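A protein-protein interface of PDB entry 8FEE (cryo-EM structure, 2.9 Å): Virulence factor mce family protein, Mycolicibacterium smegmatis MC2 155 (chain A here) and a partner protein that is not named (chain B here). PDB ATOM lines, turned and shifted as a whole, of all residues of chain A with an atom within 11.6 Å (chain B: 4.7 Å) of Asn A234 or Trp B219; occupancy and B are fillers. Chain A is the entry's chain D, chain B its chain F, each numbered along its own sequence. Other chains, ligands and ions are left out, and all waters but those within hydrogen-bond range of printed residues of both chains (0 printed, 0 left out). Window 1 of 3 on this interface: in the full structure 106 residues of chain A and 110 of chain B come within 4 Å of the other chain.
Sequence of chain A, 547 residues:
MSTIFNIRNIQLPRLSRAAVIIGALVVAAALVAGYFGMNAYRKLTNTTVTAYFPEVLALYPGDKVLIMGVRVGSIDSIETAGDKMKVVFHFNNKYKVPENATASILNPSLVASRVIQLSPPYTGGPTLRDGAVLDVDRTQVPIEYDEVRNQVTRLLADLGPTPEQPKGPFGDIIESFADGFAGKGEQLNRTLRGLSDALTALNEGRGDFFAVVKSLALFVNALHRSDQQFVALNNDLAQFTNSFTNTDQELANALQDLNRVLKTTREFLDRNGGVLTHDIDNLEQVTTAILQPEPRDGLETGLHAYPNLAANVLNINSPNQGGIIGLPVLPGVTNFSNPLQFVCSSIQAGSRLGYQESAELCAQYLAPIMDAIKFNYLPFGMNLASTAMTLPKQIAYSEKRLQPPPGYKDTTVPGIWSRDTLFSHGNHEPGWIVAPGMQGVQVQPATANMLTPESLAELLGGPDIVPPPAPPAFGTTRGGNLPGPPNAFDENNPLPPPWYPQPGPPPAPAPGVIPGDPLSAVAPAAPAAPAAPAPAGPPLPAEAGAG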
ATOM      1  N   LEU A 223     -18.125 -36.837  14.534  1.00  0.00           N
ATOM      2  CA  LEU A 223     -16.814 -36.328  14.145  1.00  0.00           C
ATOM      3  C   LEU A 223     -16.189 -37.042  12.948  1.00  0.00           C
ATOM      4  O   LEU A 223     -15.004 -36.827  12.676  1.00  0.00           O
ATOM      5  CB  LEU A 223     -15.845 -36.392  15.327  1.00  0.00           C
ATOM      6  CG  LEU A 223     -15.743 -35.142  16.199  1.00  0.00           C
ATOM      7  CD1 LEU A 223     -16.950 -35.013  17.105  1.00  0.00           C
ATOM      8  CD2 LEU A 223     -14.458 -35.163  17.006  1.00  0.00           C
ATOM      9  N   SER A 226     -15.740 -34.867   8.991  1.00  0.00           N
ATOM     10  CA  SER A 226     -14.842 -33.728   8.850  1.00  0.00           C
ATOM     11  C   SER A 226     -13.363 -34.110   8.851  1.00  0.00           C
ATOM     12  O   SER A 226     -12.542 -33.352   9.378  1.00  0.00           O
ATOM     13  CB  SER A 226     -15.125 -32.714   9.957  1.00  0.00           C
ATOM     14  OG  SER A 226     -16.488 -32.324   9.952  1.00  0.00           O
ATOM     15  N   ASP A 227     -13.003 -35.271   8.296  1.00  0.00           N
ATOM     16  CA  ASP A 227     -11.615 -35.727   8.377  1.00  0.00           C
ATOM     17  C   ASP A 227     -10.673 -34.770   7.651  1.00  0.00           C
ATOM     18  O   ASP A 227      -9.593 -34.426   8.162  1.00  0.00           O
ATOM     19  CB  ASP A 227     -11.492 -37.140   7.809  1.00  0.00           C
ATOM     20  CG  ASP A 227     -12.195 -37.294   6.478  1.00  0.00           C
ATOM     21  OD1 ASP A 227     -12.929 -36.364   6.083  1.00  0.00           O
ATOM     22  OD2 ASP A 227     -12.013 -38.342   5.825  1.00  0.00           O
ATOM     23  N   GLN A 228     -11.093 -34.280   6.480  1.00  0.00           N
ATOM     24  CA  GLN A 228     -10.269 -33.307   5.780  1.00  0.00           C
ATOM     25  C   GLN A 228     -10.259 -31.988   6.528  1.00  0.00           C
ATOM     26  O   GLN A 228      -9.263 -31.259   6.483  1.00  0.00           O
ATOM     27  CB  GLN A 228     -10.770 -33.115   4.349  1.00  0.00           C
ATOM     28  CG  GLN A 228     -10.956 -34.411   3.565  1.00  0.00           C
ATOM     29  CD  GLN A 228      -9.703 -35.271   3.522  1.00  0.00           C
ATOM     30  OE1 GLN A 228      -8.582 -34.763   3.495  1.00  0.00           O
ATOM     31  NE2 GLN A 228      -9.892 -36.585   3.517  1.00  0.00           N
ATOM     32  N   GLN A 229     -11.360 -31.660   7.212  1.00  0.00           N
ATOM     33  CA  GLN A 229     -11.382 -30.439   8.003  1.00  0.00           C
ATOM     34  C   GLN A 229     -10.363 -30.535   9.128  1.00  0.00           C
ATOM     35  O   GLN A 229      -9.719 -29.544   9.480  1.00  0.00           O
ATOM     36  CB  GLN A 229     -12.783 -30.183   8.552  1.00  0.00           C
ATOM     37  CG  GLN A 229     -13.886 -30.337   7.522  1.00  0.00           C
ATOM     38  CD  GLN A 229     -13.909 -29.202   6.522  1.00  0.00           C
ATOM     39  OE1 GLN A 229     -13.405 -28.113   6.791  1.00  0.00           O
ATOM     40  NE2 GLN A 229     -14.498 -29.451   5.358  1.00  0.00           N
ATOM     41  N   PHE A 230     -10.204 -31.731   9.703  1.00  0.00           N
ATOM     42  CA  PHE A 230      -9.232 -31.927  10.776  1.00  0.00           C
ATOM     43  C   PHE A 230      -7.807 -31.815  10.252  1.00  0.00           C
ATOM     44  O   PHE A 230      -6.936 -31.245  10.921  1.00  0.00           O
ATOM     45  CB  PHE A 230      -9.438 -33.276  11.467  1.00  0.00           C
ATOM     46  CG  PHE A 230     -10.820 -33.484  12.021  1.00  0.00           C
ATOM     47  CD1 PHE A 230     -11.650 -32.411  12.304  1.00  0.00           C
ATOM     48  CD2 PHE A 230     -11.283 -34.761  12.272  1.00  0.00           C
ATOM     49  CE1 PHE A 230     -12.914 -32.612  12.814  1.00  0.00           C
ATOM     50  CE2 PHE A 230     -12.542 -34.967  12.782  1.00  0.00           C
ATOM     51  CZ  PHE A 230     -13.360 -33.892  13.054  1.00  0.00           C
ATOM     52  N   VAL A 231      -7.549 -32.362   9.058  1.00  0.00           N
ATOM     53  CA  VAL A 231      -6.219 -32.215   8.467  1.00  0.00           C
ATOM     54  C   VAL A 231      -5.923 -30.748   8.174  1.00  0.00           C
ATOM     55  O   VAL A 231      -4.821 -30.248   8.448  1.00  0.00           O
ATOM     56  CB  VAL A 231      -6.104 -33.082   7.199  1.00  0.00           C
ATOM     57  CG1 VAL A 231      -4.773 -32.850   6.507  1.00  0.00           C
ATOM     58  CG2 VAL A 231      -6.275 -34.549   7.548  1.00  0.00           C
ATOM     59  N   ALA A 232      -6.911 -30.032   7.631  1.00  0.00           N
ATOM     60  CA  ALA A 232      -6.766 -28.600   7.398  1.00  0.00           C
ATOM     61  C   ALA A 232      -6.520 -27.853   8.701  1.00  0.00           C
ATOM     62  O   ALA A 232      -5.701 -26.931   8.749  1.00  0.00           O
ATOM     63  CB  ALA A 232      -8.005 -28.056   6.688  1.00  0.00           C
ATOM     64  N   LEU A 233      -7.227 -28.237   9.767  1.00  0.00           N
ATOM     65  CA  LEU A 233      -7.062 -27.585  11.061  1.00  0.00           C
ATOM     66  C   LEU A 233      -5.660 -27.788  11.609  1.00  0.00           C
ATOM     67  O   LEU A 233      -5.048 -26.846  12.117  1.00  0.00           O
ATOM     68  CB  LEU A 233      -8.099 -28.120  12.049  1.00  0.00           C
ATOM     69  CG  LEU A 233      -7.939 -27.762  13.528  1.00  0.00           C
ATOM     70  CD1 LEU A 233      -7.936 -26.259  13.747  1.00  0.00           C
ATOM     71  CD2 LEU A 233      -9.039 -28.419  14.344  1.00  0.00           C
ATOM     72  N   ASN A 234      -5.138 -29.011  11.520  1.00  0.00           N
ATOM     73  CA  ASN A 234      -3.795 -29.263  12.032  1.00  0.00           C
ATOM     74  C   ASN A 234      -2.744 -28.512  11.222  1.00  0.00           C
ATOM     75  O   ASN A 234      -1.799 -27.948  11.791  1.00  0.00           O
ATOM     76  CB  ASN A 234      -3.506 -30.762  12.037  1.00  0.00           C
ATOM     77  CG  ASN A 234      -4.402 -31.520  12.993  1.00  0.00           C
ATOM     78  OD1 ASN A 234      -5.180 -30.923  13.734  1.00  0.00           O
ATOM     79  ND2 ASN A 234      -4.300 -32.842  12.979  1.00  0.00           N
ATOM     80  N   ASN A 235      -2.900 -28.475   9.893  1.00  0.00           N
ATOM     81  CA  ASN A 235      -1.948 -27.728   9.074  1.00  0.00           C
ATOM     82  C   ASN A 235      -2.022 -26.228   9.351  1.00  0.00           C
ATOM     83  O   ASN A 235      -0.985 -25.559   9.444  1.00  0.00           O
ATOM     84  CB  ASN A 235      -2.191 -28.016   7.594  1.00  0.00           C
ATOM     85  CG  ASN A 235      -1.874 -29.450   7.222  1.00  0.00           C
ATOM     86  OD1 ASN A 235      -1.037 -30.096   7.852  1.00  0.00           O
ATOM     87  ND2 ASN A 235      -2.542 -29.956   6.192  1.00  0.00           N
ATOM     88  N   ASP A 236      -3.235 -25.685   9.492  1.00  0.00           N
ATOM     89  CA  ASP A 236      -3.391 -24.275   9.839  1.00  0.00           C
ATOM     90  C   ASP A 236      -2.793 -23.969  11.204  1.00  0.00           C
ATOM     91  O   ASP A 236      -2.192 -22.910  11.399  1.00  0.00           O
ATOM     92  CB  ASP A 236      -4.867 -23.880   9.801  1.00  0.00           C
ATOM     93  CG  ASP A 236      -5.446 -23.930   8.404  1.00  0.00           C
ATOM     94  OD1 ASP A 236      -4.662 -23.936   7.434  1.00  0.00           O
ATOM     95  OD2 ASP A 236      -6.687 -23.964   8.275  1.00  0.00           O
ATOM     96  N   LEU A 237      -2.970 -24.874  12.167  1.00  0.00           N
ATOM     97  CA  LEU A 237      -2.414 -24.665  13.498  1.00  0.00           C
ATOM     98  C   LEU A 237      -0.893 -24.649  13.457  1.00  0.00           C
ATOM     99  O   LEU A 237      -0.256 -23.806  14.102  1.00  0.00           O
ATOM    100  CB  LEU A 237      -2.927 -25.743  14.452  1.00  0.00           C
ATOM    101  CG  LEU A 237      -2.629 -25.575  15.940  1.00  0.00           C
ATOM    102  CD1 LEU A 237      -3.186 -24.262  16.450  1.00  0.00           C
ATOM    103  CD2 LEU A 237      -3.231 -26.732  16.709  1.00  0.00           C
ATOM    104  N   ALA A 238      -0.292 -25.575  12.705  1.00  0.00           N
ATOM    105  CA  ALA A 238       1.161 -25.575  12.567  1.00  0.00           C
ATOM    106  C   ALA A 238       1.646 -24.302  11.884  1.00  0.00           C
ATOM    107  O   ALA A 238       2.655 -23.714  12.294  1.00  0.00           O
ATOM    108  CB  ALA A 238       1.618 -26.810  11.793  1.00  0.00           C
ATOM    109  N   GLN A 239       0.933 -23.854  10.846  1.00  0.00           N
ATOM    110  CA  GLN A 239       1.303 -22.617  10.164  1.00  0.00           C
ATOM    111  C   GLN A 239       1.202 -21.417  11.098  1.00  0.00           C
ATOM    112  O   GLN A 239       2.070 -20.535  11.085  1.00  0.00           O
ATOM    113  CB  GLN A 239       0.416 -22.417   8.935  1.00  0.00           C
ATOM    114  CG  GLN A 239       0.815 -21.246   8.053  1.00  0.00           C
ATOM    115  CD  GLN A 239      -0.134 -21.050   6.885  1.00  0.00           C
ATOM    116  OE1 GLN A 239      -1.148 -21.738   6.772  1.00  0.00           O
ATOM    117  NE2 GLN A 239       0.193 -20.107   6.010  1.00  0.00           N
ATOM    118  N   PHE A 240       0.146 -21.365  11.911  1.00  0.00           N
ATOM    119  CA  PHE A 240      -0.068 -20.238  12.814  1.00  0.00           C
ATOM    120  C   PHE A 240       0.984 -20.200  13.914  1.00  0.00           C
ATOM    121  O   PHE A 240       1.538 -19.138  14.220  1.00  0.00           O
ATOM    122  CB  PHE A 240      -1.473 -20.311  13.410  1.00  0.00           C
ATOM    123  CG  PHE A 240      -1.783 -19.204  14.373  1.00  0.00           C
ATOM    124  CD1 PHE A 240      -2.002 -17.914  13.924  1.00  0.00           C
ATOM    125  CD2 PHE A 240      -1.869 -19.458  15.732  1.00  0.00           C
ATOM    126  CE1 PHE A 240      -2.289 -16.899  14.813  1.00  0.00           C
ATOM    127  CE2 PHE A 240      -2.157 -18.446  16.623  1.00  0.00           C
ATOM    128  CZ  PHE A 240      -2.367 -17.165  16.162  1.00  0.00           C
ATOM    129  N   THR A 241       1.276 -21.348  14.523  1.00  0.00           N
ATOM    130  CA  THR A 241       2.283 -21.378  15.575  1.00  0.00           C
ATOM    131  C   THR A 241       3.706 -21.292  15.039  1.00  0.00           C
ATOM    132  O   THR A 241       4.627 -21.035  15.822  1.00  0.00           O
ATOM    133  CB  THR A 241       2.130 -22.636  16.430  1.00  0.00           C
ATOM    134  OG1 THR A 241       2.450 -23.793  15.649  1.00  0.00           O
ATOM    135  CG2 THR A 241       0.713 -22.749  16.969  1.00  0.00           C
ATOM    136  N   ASN A 242       3.916 -21.503  13.737  1.00  0.00           N
ATOM    137  CA  ASN A 242       5.216 -21.207  13.147  1.00  0.00           C
ATOM    138  C   ASN A 242       5.444 -19.714  12.961  1.00  0.00           C
ATOM    139  O   ASN A 242       6.601 -19.283  12.892  1.00  0.00           O
ATOM    140  CB  ASN A 242       5.364 -21.914  11.798  1.00  0.00           C
ATOM    141  CG  ASN A 242       5.679 -23.386  11.944  1.00  0.00           C
ATOM    142  OD1 ASN A 242       6.549 -23.773  12.723  1.00  0.00           O
ATOM    143  ND2 ASN A 242       4.968 -24.219  11.195  1.00  0.00           N
ATOM    144  N   SER A 243       4.372 -18.920  12.877  1.00  0.00           N
ATOM    145  CA  SER A 243       4.505 -17.483  12.663  1.00  0.00           C
ATOM    146  C   SER A 243       5.152 -16.766  13.840  1.00  0.00           C
ATOM    147  O   SER A 243       5.715 -15.683  13.655  1.00  0.00           O
ATOM    148  CB  SER A 243       3.136 -16.865  12.378  1.00  0.00           C
ATOM    149  OG  SER A 243       2.520 -17.483  11.264  1.00  0.00           O
ATOM    150  N   PHE A 244       5.087 -17.336  15.042  1.00  0.00           N
ATOM    151  CA  PHE A 244       5.634 -16.703  16.233  1.00  0.00           C
ATOM    152  C   PHE A 244       6.864 -17.424  16.771  1.00  0.00           C
ATOM    153  O   PHE A 244       7.271 -17.168  17.907  1.00  0.00           O
ATOM    154  CB  PHE A 244       4.563 -16.613  17.322  1.00  0.00           C
ATOM    155  CG  PHE A 244       3.288 -15.967  16.865  1.00  0.00           C
ATOM    156  CD1 PHE A 244       3.213 -14.597  16.693  1.00  0.00           C
ATOM    157  CD2 PHE A 244       2.164 -16.731  16.611  1.00  0.00           C
ATOM    158  CE1 PHE A 244       2.042 -13.999  16.273  1.00  0.00           C
ATOM    159  CE2 PHE A 244       0.988 -16.139  16.192  1.00  0.00           C
ATOM    160  CZ  PHE A 244       0.928 -14.771  16.022  1.00  0.00           C
ATOM    161  N   THR A 245       7.464 -18.321  15.985  1.00  0.00           N
ATOM    162  CA  THR A 245       8.622 -19.080  16.443  1.00  0.00           C
ATOM    163  C   THR A 245       9.708 -19.145  15.377  1.00  0.00           C
ATOM    164  O   THR A 245      10.422 -20.149  15.276  1.00  0.00           O
ATOM    165  CB  THR A 245       8.226 -20.500  16.858  1.00  0.00           C
ATOM    166  OG1 THR A 245       7.269 -21.022  15.927  1.00  0.00           O
ATOM    167  CG2 THR A 245       7.630 -20.504  18.255  1.00  0.00           C
ATOM    168  N   GLN B 209      -5.997 -37.865  11.600  1.00  0.00           N
ATOM    169  CA  GLN B 209      -5.018 -37.490  12.615  1.00  0.00           C
ATOM    170  C   GLN B 209      -3.622 -37.997  12.262  1.00  0.00           C
ATOM    171  O   GLN B 209      -2.629 -37.298  12.494  1.00  0.00           O
ATOM    172  CB  GLN B 209      -5.456 -38.011  13.982  1.00  0.00           C
ATOM    173  CG  GLN B 209      -6.621 -37.253  14.592  1.00  0.00           C
ATOM    174  CD  GLN B 209      -6.329 -35.775  14.767  1.00  0.00           C
ATOM    175  OE1 GLN B 209      -5.206 -35.387  15.092  1.00  0.00           O
ATOM    176  NE2 GLN B 209      -7.339 -34.943  14.551  1.00  0.00           N
ATOM    177  N   SER B 212      -1.728 -35.943   9.519  1.00  0.00           N
ATOM    178  CA  SER B 212      -1.218 -34.650   9.953  1.00  0.00           C
ATOM    179  C   SER B 212      -0.229 -34.770  11.106  1.00  0.00           C
ATOM    180  O   SER B 212      -0.031 -33.800  11.843  1.00  0.00           O
ATOM    181  CB  SER B 212      -2.375 -33.735  10.349  1.00  0.00           C
ATOM    182  OG  SER B 212      -3.255 -33.529   9.261  1.00  0.00           O
ATOM    183  N   ALA B 215       2.428 -32.229  11.210  1.00  0.00           N
ATOM    184  CA  ALA B 215       1.888 -30.922  11.561  1.00  0.00           C
ATOM    185  C   ALA B 215       1.654 -30.819  13.059  1.00  0.00           C
ATOM    186  O   ALA B 215       1.935 -29.776  13.664  1.00  0.00           O
ATOM    187  CB  ALA B 215       0.592 -30.663  10.794  1.00  0.00           C
ATOM    188  N   ILE B 216       1.113 -31.872  13.675  1.00  0.00           N
ATOM    189  CA  ILE B 216       0.821 -31.763  15.096  1.00  0.00           C
ATOM    190  C   ILE B 216       2.115 -31.783  15.897  1.00  0.00           C
ATOM    191  O   ILE B 216       2.220 -31.098  16.919  1.00  0.00           O
ATOM    192  CB  ILE B 216      -0.184 -32.837  15.557  1.00  0.00           C
ATOM    193  CG1 ILE B 216       0.427 -34.234  15.573  1.00  0.00           C
ATOM    194  CG2 ILE B 216      -1.431 -32.808  14.687  1.00  0.00           C
ATOM    195  CD1 ILE B 216      -0.544 -35.276  16.041  1.00  0.00           C
ATOM    196  N   GLN B 217       3.125 -32.536  15.449  1.00  0.00           N
ATOM    197  CA  GLN B 217       4.429 -32.464  16.103  1.00  0.00           C
ATOM    198  C   GLN B 217       5.014 -31.061  15.997  1.00  0.00           C
ATOM    199  O   GLN B 217       5.575 -30.534  16.969  1.00  0.00           O
ATOM    200  CB  GLN B 217       5.387 -33.493  15.506  1.00  0.00           C
ATOM    201  CG  GLN B 217       5.004 -34.933  15.783  1.00  0.00           C
ATOM    202  CD  GLN B 217       6.061 -35.912  15.322  1.00  0.00           C
ATOM    203  OE1 GLN B 217       7.164 -35.518  14.942  1.00  0.00           O
ATOM    204  NE2 GLN B 217       5.730 -37.197  15.350  1.00  0.00           N
ATOM    205  N   ARG B 218       4.866 -30.426  14.827  1.00  0.00           N
ATOM    206  CA  ARG B 218       5.406 -29.082  14.652  1.00  0.00           C
ATOM    207  C   ARG B 218       4.697 -28.075  15.549  1.00  0.00           C
ATOM    208  O   ARG B 218       5.350 -27.258  16.211  1.00  0.00           O
ATOM    209  CB  ARG B 218       5.307 -28.659  13.187  1.00  0.00           C
ATOM    210  CG  ARG B 218       5.896 -27.286  12.910  1.00  0.00           C
ATOM    211  CD  ARG B 218       7.331 -27.196  13.402  1.00  0.00           C
ATOM    212  NE  ARG B 218       7.907 -25.876  13.176  1.00  0.00           N
ATOM    213  CZ  ARG B 218       9.153 -25.542  13.480  1.00  0.00           C
ATOM    214  NH1 ARG B 218       9.986 -26.410  14.031  1.00  0.00           N
ATOM    215  NH2 ARG B 218       9.574 -24.307  13.226  1.00  0.00           N
ATOM    216  N   TRP B 219       3.360 -28.108  15.593  1.00  0.00           N
ATOM    217  CA  TRP B 219       2.700 -27.125  16.446  1.00  0.00           C
ATOM    218  C   TRP B 219       2.872 -27.452  17.921  1.00  0.00           C
ATOM    219  O   TRP B 219       2.835 -26.535  18.740  1.00  0.00           O
ATOM    220  CB  TRP B 219       1.214 -26.923  16.080  1.00  0.00           C
ATOM    221  CG  TRP B 219       0.194 -28.020  16.337  1.00  0.00           C
ATOM    222  CD1 TRP B 219      -0.512 -28.693  15.384  1.00  0.00           C
ATOM    223  CD2 TRP B 219      -0.300 -28.498  17.605  1.00  0.00           C
ATOM    224  NE1 TRP B 219      -1.378 -29.583  15.968  1.00  0.00           N
ATOM    225  CE2 TRP B 219      -1.265 -29.488  17.328  1.00  0.00           C
ATOM    226  CE3 TRP B 219      -0.011 -28.200  18.940  1.00  0.00           C
ATOM    227  CZ2 TRP B 219      -1.935 -30.179  18.333  1.00  0.00           C
ATOM    228  CZ3 TRP B 219      -0.671 -28.894  19.934  1.00  0.00           C
ATOM    229  CH2 TRP B 219      -1.624 -29.869  19.626  1.00  0.00           C
ATOM    230  N   ALA B 220       3.095 -28.718  18.280  1.00  0.00           N
ATOM    231  CA  ALA B 220       3.416 -29.036  19.667  1.00  0.00           C
ATOM    232  C   ALA B 220       4.754 -28.429  20.067  1.00  0.00           C
ATOM    233  O   ALA B 220       4.877 -27.823  21.139  1.00  0.00           O
ATOM    234  CB  ALA B 220       3.425 -30.549  19.872  1.00  0.00           C
ATOM    235  N   ALA B 221       5.771 -28.576  19.210  1.00  0.00           N
ATOM    236  CA  ALA B 221       7.069 -27.971  19.506  1.00  0.00           C
ATOM    237  C   ALA B 221       6.975 -26.450  19.557  1.00  0.00           C
ATOM    238  O   ALA B 221       7.581 -25.808  20.428  1.00  0.00           O
ATOM    239  CB  ALA B 221       8.101 -28.412  18.471  1.00  0.00           C
ATOM    240  N   ASN B 222       6.210 -25.854  18.638  1.00  0.00           N
ATOM    241  CA  ASN B 222       6.055 -24.402  18.632  1.00  0.00           C
ATOM    242  C   ASN B 222       5.317 -23.911  19.872  1.00  0.00           C
ATOM    243  O   ASN B 222       5.674 -22.872  20.441  1.00  0.00           O
ATOM    244  CB  ASN B 222       5.332 -23.960  17.365  1.00  0.00           C
ATOM    245  CG  ASN B 222       6.193 -24.094  16.131  1.00  0.00           C
ATOM    246  OD1 ASN B 222       7.421 -24.140  16.218  1.00  0.00           O
ATOM    247  ND2 ASN B 222       5.556 -24.160  14.970  1.00  0.00           N
ATOM    248  N   LEU B 223       4.275 -24.631  20.293  1.00  0.00           N
ATOM    249  CA  LEU B 223       3.565 -24.271  21.513  1.00  0.00           C
ATOM    250  C   LEU B 223       4.472 -24.392  22.726  1.00  0.00           C
ATOM    251  O   LEU B 223       4.416 -23.557  23.633  1.00  0.00           O
ATOM    252  CB  LEU B 223       2.326 -25.149  21.678  1.00  0.00           C
ATOM    253  CG  LEU B 223       1.437 -24.845  22.883  1.00  0.00           C
ATOM    254  CD1 LEU B 223       0.784 -23.483  22.729  1.00  0.00           C
ATOM    255  CD2 LEU B 223       0.391 -25.930  23.068  1.00  0.00           C
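Hydrophobic or aromatic side chains of chain B that line the printed part of chain A: Ala B215, Ile B216 and Trp B219.
Among the printed residues, 16 pairs touch across the chains.
Among the printed residues, no Asp or Glu carboxylate lies within 4 Å of a Lys or Arg side-chain nitrogen of the other chain.
The side-chain hydroxyl (OG1) of Thr A241 sits at hydrogen-bond distance from the side-chain amide nitrogen (ND2) of Asn B222 (3.2 Å).
The side-chain amide nitrogen (ND2) of Asn B222 is in hydrogen-bond range of the side-chain amide oxygen (OD1) of Asn A242 (2.5 Å).
OD1 of Asn B222 sits at hydrogen-bond distance from OG1 of Thr A245 (3.1 Å).
The side-chain amide nitrogen (ND2) of Asn A234 sits at hydrogen-bond distance from the side-chain amide oxygen (OE1) of Gln B209, at 3.4 Å.
NE of Arg B218 is in hydrogen-bond range of OD1 of Asn A242 (2.5 Å).
The backbone carbonyl oxygen (O) of Phe A230 lies close to the side-chain amide oxygen (OD1) of Asn A234, at 3.3 Å.
The side-chain hydroxyl of Thr A245 lies within hydrogen-bond range of the backbone carbonyl oxygen of Thr A241 (2.6 Å).
The side-chain amide nitrogen (ND2) of Asn B222 lies close to the backbone carbonyl oxygen (O) of Arg B218, 3.3 Å away.
O of Ala A238 sits at hydrogen-bond distance from OG1 of Thr A241 (3.4 Å).
ND2 of Asn A235 lies within hydrogen-bond range of O of Val A231, 3.2 Å away.
The backbone carbonyl oxygen of Leu A237 is in hydrogen-bond range of the side-chain hydroxyl of Thr A241 (3.1 Å).
Printed residues of chain B within 4 Å of Val A231: Ser B212 (3.2 Å).
Of the printed residues of chain B, Thr A245 touches Asn B222 (3.1 Å).
Gln B209 touches just one residue of chain A: Asn A234.
Of the printed residues of chain A, Ser B212 touches Val A231 (3.2 Å) and Asn A234 (3.4 Å).
Ala B215 touches three residues of chain A.
Of chain A, only Asn A234 (3.3 Å) comes within 4 Å of Ile B216.
Of the printed residues of chain A, Arg B218 touches Asn A242.
Trp B219 touches just these residues of chain A: Asn A234 (3.9 Å), Leu A237 (3.4 Å), Ala A238 (3.8 Å) and Thr A241 (3.4 Å).
No residue of chain A comes within 4 Å of Ala B220.
No residue of chain A comes within 4 Å of Ala B221.
No residue of chain A comes within 4 Å of Leu B223.
The nearest printed residue of chain B that does not touch Asn A234 is Arg B218 (7.3 Å).
The nearest residue of chain A that does not touch Trp B219 is Leu A233 (5.9 Å).
The nearest printed residue of chain B that does not touch Ala A238 is Arg B218 (4.4 Å).
CG1 of Val A231 touches OG of Ser B212, 3.2 Å away.
CB of Ser B212 touches ND2 of Asn A234, 3.4 Å away.
Ala B215 touches Asn A234.
CG2 of Ile B216 touches ND2 of Asn A234, 3.3 Å away.
Asn A234 touches Trp B219.
Asn A235 touches Ala B215 (OD1 to CB, 3.4 Å).
Leu A237 touches Trp B219 (CD2 to CE2, 3.4 Å).
CB of Ala A238 touches O of Ala B215, 3.5 Å away.
ND2 of Asn B222 touches O of Ala A238, at 3.97 Å.
Thr A241 touches Trp B219.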
